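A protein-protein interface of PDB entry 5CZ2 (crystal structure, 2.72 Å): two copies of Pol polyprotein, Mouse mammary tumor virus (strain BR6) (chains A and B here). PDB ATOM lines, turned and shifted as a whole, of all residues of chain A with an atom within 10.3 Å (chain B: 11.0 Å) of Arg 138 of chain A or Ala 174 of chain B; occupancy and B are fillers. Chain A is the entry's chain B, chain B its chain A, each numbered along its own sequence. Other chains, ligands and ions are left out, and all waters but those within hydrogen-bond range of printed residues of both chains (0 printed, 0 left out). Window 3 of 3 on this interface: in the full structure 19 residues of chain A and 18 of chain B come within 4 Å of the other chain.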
ATOM      1  N   LEU A 103      -5.583  -4.156 -33.245  1.00  0.00           N
ATOM      2  CA  LEU A 103      -4.629  -4.631 -32.246  1.00  0.00           C
ATOM      3  C   LEU A 103      -5.091  -4.302 -30.833  1.00  0.00           C
ATOM      4  O   LEU A 103      -4.986  -5.138 -29.928  1.00  0.00           O
ATOM      5  CB  LEU A 103      -3.249  -4.031 -32.514  1.00  0.00           C
ATOM      6  CG  LEU A 103      -2.463  -4.672 -33.657  1.00  0.00           C
ATOM      7  CD1 LEU A 103      -1.202  -3.884 -33.957  1.00  0.00           C
ATOM      8  CD2 LEU A 103      -2.122  -6.107 -33.302  1.00  0.00           C
ATOM      9  N   PHE A 110      -8.760 -10.159 -25.139  1.00  0.00           N
ATOM     10  CA  PHE A 110      -8.065 -11.193 -24.377  1.00  0.00           C
ATOM     11  C   PHE A 110      -8.281 -11.019 -22.880  1.00  0.00           C
ATOM     12  O   PHE A 110      -8.491 -12.003 -22.159  1.00  0.00           O
ATOM     13  CB  PHE A 110      -6.573 -11.183 -24.710  1.00  0.00           C
ATOM     14  CG  PHE A 110      -6.268 -11.515 -26.144  1.00  0.00           C
ATOM     15  CD1 PHE A 110      -7.183 -12.208 -26.920  1.00  0.00           C
ATOM     16  CD2 PHE A 110      -5.063 -11.140 -26.713  1.00  0.00           C
ATOM     17  CE1 PHE A 110      -6.903 -12.515 -28.236  1.00  0.00           C
ATOM     18  CE2 PHE A 110      -4.776 -11.444 -28.029  1.00  0.00           C
ATOM     19  CZ  PHE A 110      -5.698 -12.133 -28.793  1.00  0.00           C
ATOM     20  N   ILE A 115      -7.713 -16.358 -24.048  1.00  0.00           N
ATOM     21  CA  ILE A 115      -6.996 -16.647 -25.289  1.00  0.00           C
ATOM     22  C   ILE A 115      -7.731 -17.754 -26.036  1.00  0.00           C
ATOM     23  O   ILE A 115      -8.018 -18.799 -25.440  1.00  0.00           O
ATOM     24  CB  ILE A 115      -5.533 -17.049 -25.030  1.00  0.00           C
ATOM     25  CG1 ILE A 115      -4.713 -15.815 -24.671  1.00  0.00           C
ATOM     26  CG2 ILE A 115      -4.938 -17.743 -26.242  1.00  0.00           C
ATOM     27  CD1 ILE A 115      -4.760 -14.732 -25.724  1.00  0.00           C
ATOM     28  N   PRO A 116      -8.046 -17.570 -27.312  1.00  0.00           N
ATOM     29  CA  PRO A 116      -8.552 -18.669 -28.135  1.00  0.00           C
ATOM     30  C   PRO A 116      -7.411 -19.387 -28.848  1.00  0.00           C
ATOM     31  O   PRO A 116      -6.279 -18.905 -28.916  1.00  0.00           O
ATOM     32  CB  PRO A 116      -9.448 -17.944 -29.144  1.00  0.00           C
ATOM     33  CG  PRO A 116      -8.728 -16.645 -29.359  1.00  0.00           C
ATOM     34  CD  PRO A 116      -8.073 -16.287 -28.038  1.00  0.00           C
ATOM     35  N   ARG A 130       0.424  -7.333 -41.881  1.00  0.00           N
ATOM     36  CA  ARG A 130       1.562  -8.025 -41.285  1.00  0.00           C
ATOM     37  C   ARG A 130       1.625  -7.806 -39.781  1.00  0.00           C
ATOM     38  O   ARG A 130       2.097  -8.685 -39.049  1.00  0.00           O
ATOM     39  CB  ARG A 130       2.862  -7.564 -41.943  1.00  0.00           C
ATOM     40  N   SER A 131       1.164  -6.648 -39.303  1.00  0.00           N
ATOM     41  CA  SER A 131       1.135  -6.406 -37.865  1.00  0.00           C
ATOM     42  C   SER A 131       0.230  -7.408 -37.162  1.00  0.00           C
ATOM     43  O   SER A 131       0.583  -7.935 -36.101  1.00  0.00           O
ATOM     44  CB  SER A 131       0.680  -4.976 -37.581  1.00  0.00           C
ATOM     45  OG  SER A 131       1.251  -4.064 -38.503  1.00  0.00           O
ATOM     46  N   ILE A 132      -0.936  -7.692 -37.743  1.00  0.00           N
ATOM     47  CA  ILE A 132      -1.843  -8.667 -37.146  1.00  0.00           C
ATOM     48  C   ILE A 132      -1.248 -10.065 -37.233  1.00  0.00           C
ATOM     49  O   ILE A 132      -1.312 -10.841 -36.272  1.00  0.00           O
ATOM     50  CB  ILE A 132      -3.225  -8.595 -37.819  1.00  0.00           C
ATOM     51  CG1 ILE A 132      -3.786  -7.177 -37.733  1.00  0.00           C
ATOM     52  CG2 ILE A 132      -4.184  -9.583 -37.176  1.00  0.00           C
ATOM     53  CD1 ILE A 132      -3.979  -6.684 -36.326  1.00  0.00           C
ATOM     54  N   GLN A 133      -0.668 -10.412 -38.385  1.00  0.00           N
ATOM     55  CA  GLN A 133      -0.057 -11.729 -38.546  1.00  0.00           C
ATOM     56  C   GLN A 133       1.055 -11.954 -37.527  1.00  0.00           C
ATOM     57  O   GLN A 133       1.100 -12.994 -36.860  1.00  0.00           O
ATOM     58  CB  GLN A 133       0.477 -11.887 -39.969  1.00  0.00           C
ATOM     59  CG  GLN A 133      -0.604 -12.018 -41.030  1.00  0.00           C
ATOM     60  CD  GLN A 133      -0.032 -12.197 -42.424  1.00  0.00           C
ATOM     61  OE1 GLN A 133       1.041 -11.683 -42.740  1.00  0.00           O
ATOM     62  NE2 GLN A 133      -0.748 -12.936 -43.266  1.00  0.00           N
ATOM     63  N   GLU A 134       1.963 -10.987 -37.390  1.00  0.00           N
ATOM     64  CA  GLU A 134       3.079 -11.139 -36.465  1.00  0.00           C
ATOM     65  C   GLU A 134       2.675 -10.956 -35.007  1.00  0.00           C
ATOM     66  O   GLU A 134       3.361 -11.475 -34.121  1.00  0.00           O
ATOM     67  CB  GLU A 134       4.197 -10.157 -36.823  1.00  0.00           C
ATOM     68  CG  GLU A 134       4.855 -10.455 -38.160  1.00  0.00           C
ATOM     69  CD  GLU A 134       6.028  -9.543 -38.452  1.00  0.00           C
ATOM     70  OE1 GLU A 134       6.153  -8.498 -37.779  1.00  0.00           O
ATOM     71  OE2 GLU A 134       6.828  -9.874 -39.351  1.00  0.00           O
ATOM     72  N   PHE A 135       1.588 -10.230 -34.738  1.00  0.00           N
ATOM     73  CA  PHE A 135       1.080 -10.136 -33.372  1.00  0.00           C
ATOM     74  C   PHE A 135       0.531 -11.477 -32.903  1.00  0.00           C
ATOM     75  O   PHE A 135       0.892 -11.966 -31.825  1.00  0.00           O
ATOM     76  CB  PHE A 135       0.008  -9.047 -33.287  1.00  0.00           C
ATOM     77  CG  PHE A 135      -0.727  -9.011 -31.978  1.00  0.00           C
ATOM     78  CD1 PHE A 135      -0.148  -8.441 -30.857  1.00  0.00           C
ATOM     79  CD2 PHE A 135      -2.008  -9.530 -31.873  1.00  0.00           C
ATOM     80  CE1 PHE A 135      -0.827  -8.402 -29.654  1.00  0.00           C
ATOM     81  CE2 PHE A 135      -2.691  -9.494 -30.673  1.00  0.00           C
ATOM     82  CZ  PHE A 135      -2.100  -8.928 -29.562  1.00  0.00           C
ATOM     83  N   LEU A 136      -0.349 -12.085 -33.703  1.00  0.00           N
ATOM     84  CA  LEU A 136      -0.907 -13.386 -33.353  1.00  0.00           C
ATOM     85  C   LEU A 136       0.161 -14.471 -33.324  1.00  0.00           C
ATOM     86  O   LEU A 136      -0.003 -15.486 -32.638  1.00  0.00           O
ATOM     87  CB  LEU A 136      -2.018 -13.761 -34.336  1.00  0.00           C
ATOM     88  CG  LEU A 136      -3.193 -12.786 -34.445  1.00  0.00           C
ATOM     89  CD1 LEU A 136      -4.159 -13.225 -35.536  1.00  0.00           C
ATOM     90  CD2 LEU A 136      -3.909 -12.656 -33.112  1.00  0.00           C
ATOM     91  N   ALA A 137       1.257 -14.280 -34.063  1.00  0.00           N
ATOM     92  CA  ALA A 137       2.333 -15.267 -34.070  1.00  0.00           C
ATOM     93  C   ALA A 137       2.989 -15.383 -32.700  1.00  0.00           C
ATOM     94  O   ALA A 137       3.196 -16.491 -32.191  1.00  0.00           O
ATOM     95  CB  ALA A 137       3.367 -14.904 -35.136  1.00  0.00           C
ATOM     96  N   ARG A 138       3.330 -14.246 -32.089  1.00  0.00           N
ATOM     97  CA  ARG A 138       3.909 -14.276 -30.750  1.00  0.00           C
ATOM     98  C   ARG A 138       2.931 -14.858 -29.735  1.00  0.00           C
ATOM     99  O   ARG A 138       3.333 -15.585 -28.820  1.00  0.00           O
ATOM    100  CB  ARG A 138       4.339 -12.872 -30.326  1.00  0.00           C
ATOM    101  CG  ARG A 138       5.429 -12.259 -31.186  1.00  0.00           C
ATOM    102  CD  ARG A 138       6.050 -11.062 -30.487  1.00  0.00           C
ATOM    103  NE  ARG A 138       6.673 -11.445 -29.224  1.00  0.00           N
ATOM    104  CZ  ARG A 138       7.157 -10.584 -28.335  1.00  0.00           C
ATOM    105  NH1 ARG A 138       7.088  -9.281 -28.564  1.00  0.00           N
ATOM    106  NH2 ARG A 138       7.707 -11.028 -27.212  1.00  0.00           N
ATOM    107  N   TRP A 139       1.642 -14.551 -29.886  1.00  0.00           N
ATOM    108  CA  TRP A 139       0.618 -15.039 -28.971  1.00  0.00           C
ATOM    109  C   TRP A 139       0.290 -16.514 -29.167  1.00  0.00           C
ATOM    110  O   TRP A 139      -0.527 -17.045 -28.408  1.00  0.00           O
ATOM    111  CB  TRP A 139      -0.655 -14.204 -29.128  1.00  0.00           C
ATOM    112  CG  TRP A 139      -0.927 -13.291 -27.972  1.00  0.00           C
ATOM    113  CD1 TRP A 139      -1.881 -13.450 -27.011  1.00  0.00           C
ATOM    114  CD2 TRP A 139      -0.232 -12.081 -27.650  1.00  0.00           C
ATOM    115  NE1 TRP A 139      -1.828 -12.413 -26.113  1.00  0.00           N
ATOM    116  CE2 TRP A 139      -0.823 -11.558 -26.483  1.00  0.00           C
ATOM    117  CE3 TRP A 139       0.831 -11.389 -28.235  1.00  0.00           C
ATOM    118  CZ2 TRP A 139      -0.386 -10.377 -25.890  1.00  0.00           C
ATOM    119  CZ3 TRP A 139       1.263 -10.214 -27.645  1.00  0.00           C
ATOM    120  CH2 TRP A 139       0.655  -9.721 -26.486  1.00  0.00           C
ATOM    121  N   LYS A 140       0.903 -17.177 -30.151  1.00  0.00           N
ATOM    122  CA  LYS A 140       0.635 -18.585 -30.459  1.00  0.00           C
ATOM    123  C   LYS A 140      -0.851 -18.814 -30.734  1.00  0.00           C
ATOM    124  O   LYS A 140      -1.475 -19.731 -30.195  1.00  0.00           O
ATOM    125  CB  LYS A 140       1.138 -19.504 -29.342  1.00  0.00           C
ATOM    126  CG  LYS A 140       2.632 -19.405 -29.074  1.00  0.00           C
ATOM    127  CD  LYS A 140       3.104 -20.534 -28.168  1.00  0.00           C
ATOM    128  CE  LYS A 140       2.355 -20.544 -26.844  1.00  0.00           C
ATOM    129  NZ  LYS A 140       2.610 -19.314 -26.044  1.00  0.00           N
ATOM    130  N   ILE A 141      -1.417 -17.965 -31.588  1.00  0.00           N
ATOM    131  CA  ILE A 141      -2.824 -18.026 -31.962  1.00  0.00           C
ATOM    132  C   ILE A 141      -2.912 -18.186 -33.473  1.00  0.00           C
ATOM    133  O   ILE A 141      -2.339 -17.385 -34.221  1.00  0.00           O
ATOM    134  CB  ILE A 141      -3.587 -16.769 -31.502  1.00  0.00           C
ATOM    135  CG1 ILE A 141      -3.488 -16.608 -29.983  1.00  0.00           C
ATOM    136  CG2 ILE A 141      -5.042 -16.835 -31.941  1.00  0.00           C
ATOM    137  CD1 ILE A 141      -4.188 -15.374 -29.456  1.00  0.00           C
ATOM    138  N   SER A 142      -3.623 -19.218 -33.919  1.00  0.00           N
ATOM    139  CA  SER A 142      -3.810 -19.441 -35.344  1.00  0.00           C
ATOM    140  C   SER A 142      -4.899 -18.526 -35.889  1.00  0.00           C
ATOM    141  O   SER A 142      -5.827 -18.133 -35.177  1.00  0.00           O
ATOM    142  CB  SER A 142      -4.165 -20.902 -35.621  1.00  0.00           C
ATOM    143  OG  SER A 142      -3.112 -21.766 -35.232  1.00  0.00           O
ATOM    144  N   ALA B 166       2.992  -3.532 -10.800  1.00  0.00           N
ATOM    145  CA  ALA B 166       4.086  -4.475 -11.003  1.00  0.00           C
ATOM    146  C   ALA B 166       4.029  -5.086 -12.398  1.00  0.00           C
ATOM    147  O   ALA B 166       5.040  -5.136 -13.108  1.00  0.00           O
ATOM    148  CB  ALA B 166       4.045  -5.566  -9.932  1.00  0.00           C
ATOM    149  N   GLN B 167       2.847  -5.553 -12.809  1.00  0.00           N
ATOM    150  CA  GLN B 167       2.710  -6.165 -14.128  1.00  0.00           C
ATOM    151  C   GLN B 167       2.923  -5.147 -15.241  1.00  0.00           C
ATOM    152  O   GLN B 167       3.492  -5.478 -16.289  1.00  0.00           O
ATOM    153  CB  GLN B 167       1.337  -6.823 -14.262  1.00  0.00           C
ATOM    154  CG  GLN B 167       1.344  -8.325 -14.027  1.00  0.00           C
ATOM    155  CD  GLN B 167       2.115  -9.076 -15.094  1.00  0.00           C
ATOM    156  OE1 GLN B 167       1.993  -8.786 -16.285  1.00  0.00           O
ATOM    157  NE2 GLN B 167       2.913 -10.050 -14.674  1.00  0.00           N
ATOM    158  N   LEU B 168       2.469  -3.906 -15.039  1.00  0.00           N
ATOM    159  CA  LEU B 168       2.669  -2.873 -16.052  1.00  0.00           C
ATOM    160  C   LEU B 168       4.150  -2.642 -16.324  1.00  0.00           C
ATOM    161  O   LEU B 168       4.563  -2.524 -17.483  1.00  0.00           O
ATOM    162  CB  LEU B 168       1.993  -1.570 -15.621  1.00  0.00           C
ATOM    163  CG  LEU B 168       0.464  -1.562 -15.641  1.00  0.00           C
ATOM    164  CD1 LEU B 168      -0.072  -0.289 -15.006  1.00  0.00           C
ATOM    165  CD2 LEU B 168      -0.060  -1.719 -17.060  1.00  0.00           C
ATOM    166  N   ASN B 169       4.964  -2.571 -15.267  1.00  0.00           N
ATOM    167  CA  ASN B 169       6.396  -2.347 -15.444  1.00  0.00           C
ATOM    168  C   ASN B 169       7.036  -3.465 -16.257  1.00  0.00           C
ATOM    169  O   ASN B 169       7.875  -3.207 -17.128  1.00  0.00           O
ATOM    170  CB  ASN B 169       7.080  -2.215 -14.084  1.00  0.00           C
ATOM    171  CG  ASN B 169       7.205  -0.773 -13.634  1.00  0.00           C
ATOM    172  OD1 ASN B 169       8.246  -0.142 -13.818  1.00  0.00           O
ATOM    173  ND2 ASN B 169       6.144  -0.244 -13.037  1.00  0.00           N
ATOM    174  N   LYS B 170       6.655  -4.716 -15.981  1.00  0.00           N
ATOM    175  CA  LYS B 170       7.267  -5.851 -16.666  1.00  0.00           C
ATOM    176  C   LYS B 170       6.977  -5.842 -18.162  1.00  0.00           C
ATOM    177  O   LYS B 170       7.788  -6.340 -18.952  1.00  0.00           O
ATOM    178  CB  LYS B 170       6.776  -7.161 -16.048  1.00  0.00           C
ATOM    179  CG  LYS B 170       6.912  -7.239 -14.537  1.00  0.00           C
ATOM    180  CD  LYS B 170       6.613  -8.640 -14.034  1.00  0.00           C
ATOM    181  CE  LYS B 170       5.852  -8.606 -12.720  1.00  0.00           C
ATOM    182  NZ  LYS B 170       5.931  -9.905 -11.995  1.00  0.00           N
ATOM    183  N   LEU B 171       5.835  -5.287 -18.571  1.00  0.00           N
ATOM    184  CA  LEU B 171       5.377  -5.436 -19.947  1.00  0.00           C
ATOM    185  C   LEU B 171       6.061  -4.482 -20.922  1.00  0.00           C
ATOM    186  O   LEU B 171       6.095  -4.774 -22.123  1.00  0.00           O
ATOM    187  CB  LEU B 171       3.861  -5.243 -20.015  1.00  0.00           C
ATOM    188  CG  LEU B 171       3.029  -6.389 -19.432  1.00  0.00           C
ATOM    189  CD1 LEU B 171       1.547  -6.163 -19.681  1.00  0.00           C
ATOM    190  CD2 LEU B 171       3.476  -7.728 -20.002  1.00  0.00           C
ATOM    191  N   GLN B 172       6.593  -3.353 -20.443  1.00  0.00           N
ATOM    192  CA  GLN B 172       7.301  -2.429 -21.328  1.00  0.00           C
ATOM    193  C   GLN B 172       8.497  -3.103 -21.989  1.00  0.00           C
ATOM    194  O   GLN B 172       8.680  -3.018 -23.209  1.00  0.00           O
ATOM    195  CB  GLN B 172       7.754  -1.193 -20.548  1.00  0.00           C
ATOM    196  CG  GLN B 172       6.911   0.055 -20.771  1.00  0.00           C
ATOM    197  CD  GLN B 172       5.651   0.067 -19.934  1.00  0.00           C
ATOM    198  OE1 GLN B 172       5.057  -0.976 -19.669  1.00  0.00           O
ATOM    199  NE2 GLN B 172       5.239   1.254 -19.505  1.00  0.00           N
ATOM    200  N   LYS B 173       9.323  -3.783 -21.192  1.00  0.00           N
ATOM    201  CA  LYS B 173      10.578  -4.342 -21.679  1.00  0.00           C
ATOM    202  C   LYS B 173      10.378  -5.453 -22.702  1.00  0.00           C
ATOM    203  O   LYS B 173      11.344  -5.832 -23.374  1.00  0.00           O
ATOM    204  CB  LYS B 173      11.412  -4.867 -20.506  1.00  0.00           C
ATOM    205  CG  LYS B 173      11.987  -3.798 -19.569  1.00  0.00           C
ATOM    206  CD  LYS B 173      10.927  -3.180 -18.661  1.00  0.00           C
ATOM    207  CE  LYS B 173      11.501  -2.772 -17.317  1.00  0.00           C
ATOM    208  NZ  LYS B 173      11.819  -3.960 -16.479  1.00  0.00           N
ATOM    209  N   ALA B 174       9.159  -5.980 -22.839  1.00  0.00           N
ATOM    210  CA  ALA B 174       8.902  -7.000 -23.849  1.00  0.00           C
ATOM    211  C   ALA B 174       8.668  -6.379 -25.221  1.00  0.00           C
ATOM    212  O   ALA B 174       9.076  -6.948 -26.240  1.00  0.00           O
ATOM    213  CB  ALA B 174       7.703  -7.856 -23.439  1.00  0.00           C
ATOM    214  N   GLY B 175       8.021  -5.223 -25.264  1.00  0.00           N
ATOM    215  CA  GLY B 175       7.757  -4.557 -26.527  1.00  0.00           C
ATOM    216  C   GLY B 175       7.009  -3.265 -26.291  1.00  0.00           C
ATOM    217  O   GLY B 175       6.551  -2.974 -25.180  1.00  0.00           O
ATOM    218  N   LYS B 176       6.890  -2.490 -27.363  1.00  0.00           N
ATOM    219  CA  LYS B 176       6.194  -1.214 -27.326  1.00  0.00           C
ATOM    220  C   LYS B 176       4.696  -1.414 -27.527  1.00  0.00           C
ATOM    221  O   LYS B 176       4.259  -2.299 -28.268  1.00  0.00           O
ATOM    222  CB  LYS B 176       6.740  -0.268 -28.396  1.00  0.00           C
ATOM    223  N   TYR B 177       3.912  -0.577 -26.856  1.00  0.00           N
ATOM    224  CA  TYR B 177       2.461  -0.594 -26.958  1.00  0.00           C
ATOM    225  C   TYR B 177       1.974   0.701 -27.596  1.00  0.00           C
ATOM    226  O   TYR B 177       2.732   1.656 -27.785  1.00  0.00           O
ATOM    227  CB  TYR B 177       1.818  -0.790 -25.580  1.00  0.00           C
ATOM    228  CG  TYR B 177       2.112  -2.132 -24.947  1.00  0.00           C
ATOM    229  CD1 TYR B 177       1.287  -3.226 -25.179  1.00  0.00           C
ATOM    230  CD2 TYR B 177       3.212  -2.306 -24.119  1.00  0.00           C
ATOM    231  CE1 TYR B 177       1.551  -4.455 -24.603  1.00  0.00           C
ATOM    232  CE2 TYR B 177       3.484  -3.531 -23.538  1.00  0.00           C
ATOM    233  CZ  TYR B 177       2.650  -4.601 -23.784  1.00  0.00           C
ATOM    234  OH  TYR B 177       2.916  -5.822 -23.210  1.00  0.00           O
ATOM    235  N   HIS B 182      -3.920  -0.204 -24.357  1.00  0.00           N
ATOM    236  CA  HIS B 182      -3.273  -1.418 -24.845  1.00  0.00           C
ATOM    237  C   HIS B 182      -2.466  -2.085 -23.740  1.00  0.00           C
ATOM    238  O   HIS B 182      -2.601  -3.289 -23.493  1.00  0.00           O
ATOM    239  CB  HIS B 182      -2.381  -1.082 -26.042  1.00  0.00           C
ATOM    240  CG  HIS B 182      -2.025  -2.265 -26.887  1.00  0.00           C
ATOM    241  ND1 HIS B 182      -2.056  -3.558 -26.413  1.00  0.00           N
ATOM    242  CD2 HIS B 182      -1.621  -2.348 -28.177  1.00  0.00           C
ATOM    243  CE1 HIS B 182      -1.691  -4.387 -27.374  1.00  0.00           C
ATOM    244  NE2 HIS B 182      -1.421  -3.677 -28.455  1.00  0.00           N
ATOM    245  N   LEU B 183      -1.608  -1.312 -23.071  1.00  0.00           N
ATOM    246  CA  LEU B 183      -0.790  -1.848 -21.988  1.00  0.00           C
ATOM    247  C   LEU B 183      -1.656  -2.438 -20.882  1.00  0.00           C
ATOM    248  O   LEU B 183      -1.386  -3.535 -20.380  1.00  0.00           O
ATOM    249  CB  LEU B 183       0.110  -0.745 -21.434  1.00  0.00           C
ATOM    250  CG  LEU B 183       1.575  -1.056 -21.130  1.00  0.00           C
ATOM    251  CD1 LEU B 183       2.224   0.167 -20.512  1.00  0.00           C
ATOM    252  CD2 LEU B 183       1.715  -2.264 -20.219  1.00  0.00           C
ATOM    253  N   HIS B 186      -3.384  -5.819 -21.633  1.00  0.00           N
ATOM    254  CA  HIS B 186      -2.452  -6.938 -21.524  1.00  0.00           C
ATOM    255  C   HIS B 186      -2.192  -7.296 -20.065  1.00  0.00           C
ATOM    256  O   HIS B 186      -2.201  -8.474 -19.692  1.00  0.00           O
ATOM    257  CB  HIS B 186      -1.144  -6.596 -22.243  1.00  0.00           C
ATOM    258  CG  HIS B 186      -0.245  -7.774 -22.469  1.00  0.00           C
ATOM    259  ND1 HIS B 186       0.824  -7.735 -23.338  1.00  0.00           N
ATOM    260  CD2 HIS B 186      -0.258  -9.022 -21.946  1.00  0.00           C
ATOM    261  CE1 HIS B 186       1.435  -8.906 -23.336  1.00  0.00           C
ATOM    262  NE2 HIS B 186       0.797  -9.706 -22.500  1.00  0.00           N
ATOM    263  N   ALA B 187      -1.952  -6.284 -19.226  1.00  0.00           N
ATOM    264  CA  ALA B 187      -1.736  -6.521 -17.801  1.00  0.00           C
ATOM    265  C   ALA B 187      -2.921  -7.243 -17.168  1.00  0.00           C
ATOM    266  O   ALA B 187      -2.744  -8.203 -16.410  1.00  0.00           O
ATOM    267  CB  ALA B 187      -1.467  -5.197 -17.087  1.00  0.00           C
ATOM    268  N   PHE B 189      -5.162  -9.126 -18.616  1.00  0.00           N
ATOM    269  CA  PHE B 189      -5.208 -10.492 -19.131  1.00  0.00           C
ATOM    270  C   PHE B 189      -4.311 -11.430 -18.330  1.00  0.00           C
ATOM    271  O   PHE B 189      -4.714 -12.552 -17.999  1.00  0.00           O
ATOM    272  CB  PHE B 189      -4.813 -10.499 -20.607  1.00  0.00           C
ATOM    273  CG  PHE B 189      -4.349 -11.834 -21.103  1.00  0.00           C
ATOM    274  CD1 PHE B 189      -5.220 -12.906 -21.173  1.00  0.00           C
ATOM    275  CD2 PHE B 189      -3.033 -12.017 -21.490  1.00  0.00           C
ATOM    276  CE1 PHE B 189      -4.786 -14.135 -21.624  1.00  0.00           C
ATOM    277  CE2 PHE B 189      -2.594 -13.243 -21.944  1.00  0.00           C
ATOM    278  CZ  PHE B 189      -3.470 -14.301 -22.010  1.00  0.00           C
ATOM    279  N   VAL B 190      -3.093 -10.992 -18.007  1.00  0.00           N
ATOM    280  CA  VAL B 190      -2.154 -11.859 -17.300  1.00  0.00           C
ATOM    281  C   VAL B 190      -2.627 -12.111 -15.874  1.00  0.00           C
ATOM    282  O   VAL B 190      -2.664 -13.257 -15.408  1.00  0.00           O
ATOM    283  CB  VAL B 190      -0.738 -11.255 -17.324  1.00  0.00           C
ATOM    284  CG1 VAL B 190       0.243 -12.173 -16.609  1.00  0.00           C
ATOM    285  CG2 VAL B 190      -0.290 -11.003 -18.755  1.00  0.00           C
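The side-chain hydroxyl (OH) of Tyr 177 of chain B lies within hydrogen-bond range of a ring nitrogen (ND1) of His 186 of chain B, 2.8 Å away.
Phe 110 of chain A touches Phe 189 of chain B.
CG1 of Ile 115 of chain A touches CZ of Phe 189 of chain B, 3.3 Å away.
O of Ala 174 of chain B touches NH1 of Arg 138 of chain A (3.8 Å).
Trp 139 of chain A touches His 186 of chain B (CH2 to CE1, 3.3 Å).
Of the printed residues of chain B, Ile 115 of chain A touches Phe 189.
No residue of chain B comes within 4 Å of Ala 137 of chain A.
Of the printed residues of chain B, Arg 138 of chain A touches Ala 174.
Of chain B, only His 186 (3.3 Å) comes within 4 Å of Trp 139 of chain A.
No residue of chain B comes within 4 Å of Lys 140 of chain A.
No residue of chain A comes within 4 Å of Gly 175 of chain B.
Printed residues of chain A within 4 Å of Phe 189 of chain B: Phe 110 (3.5 Å) and Ile 115 (3.3 Å).
Of the 17 printed residues of chain A, 4 touch a printed residue of chain B.
Printed residues of chain A that touch a printed residue of chain B: Phe 110, Ile 115, Arg 138 and Trp 139.
Hydrophobic or aromatic side chains of chain A that line the printed part of chain B: Ile 115 and Trp 139.
Hydrophobic or aromatic side chains of chain B that line the printed part of chain A: His 186 and Phe 189.
Among the printed residues, 4 pairs touch across the chains.
No position is printed for both chains.
Of the 4 pairs that touch across the chains among the printed residues, none has its exchanged pair printed and touching as well.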
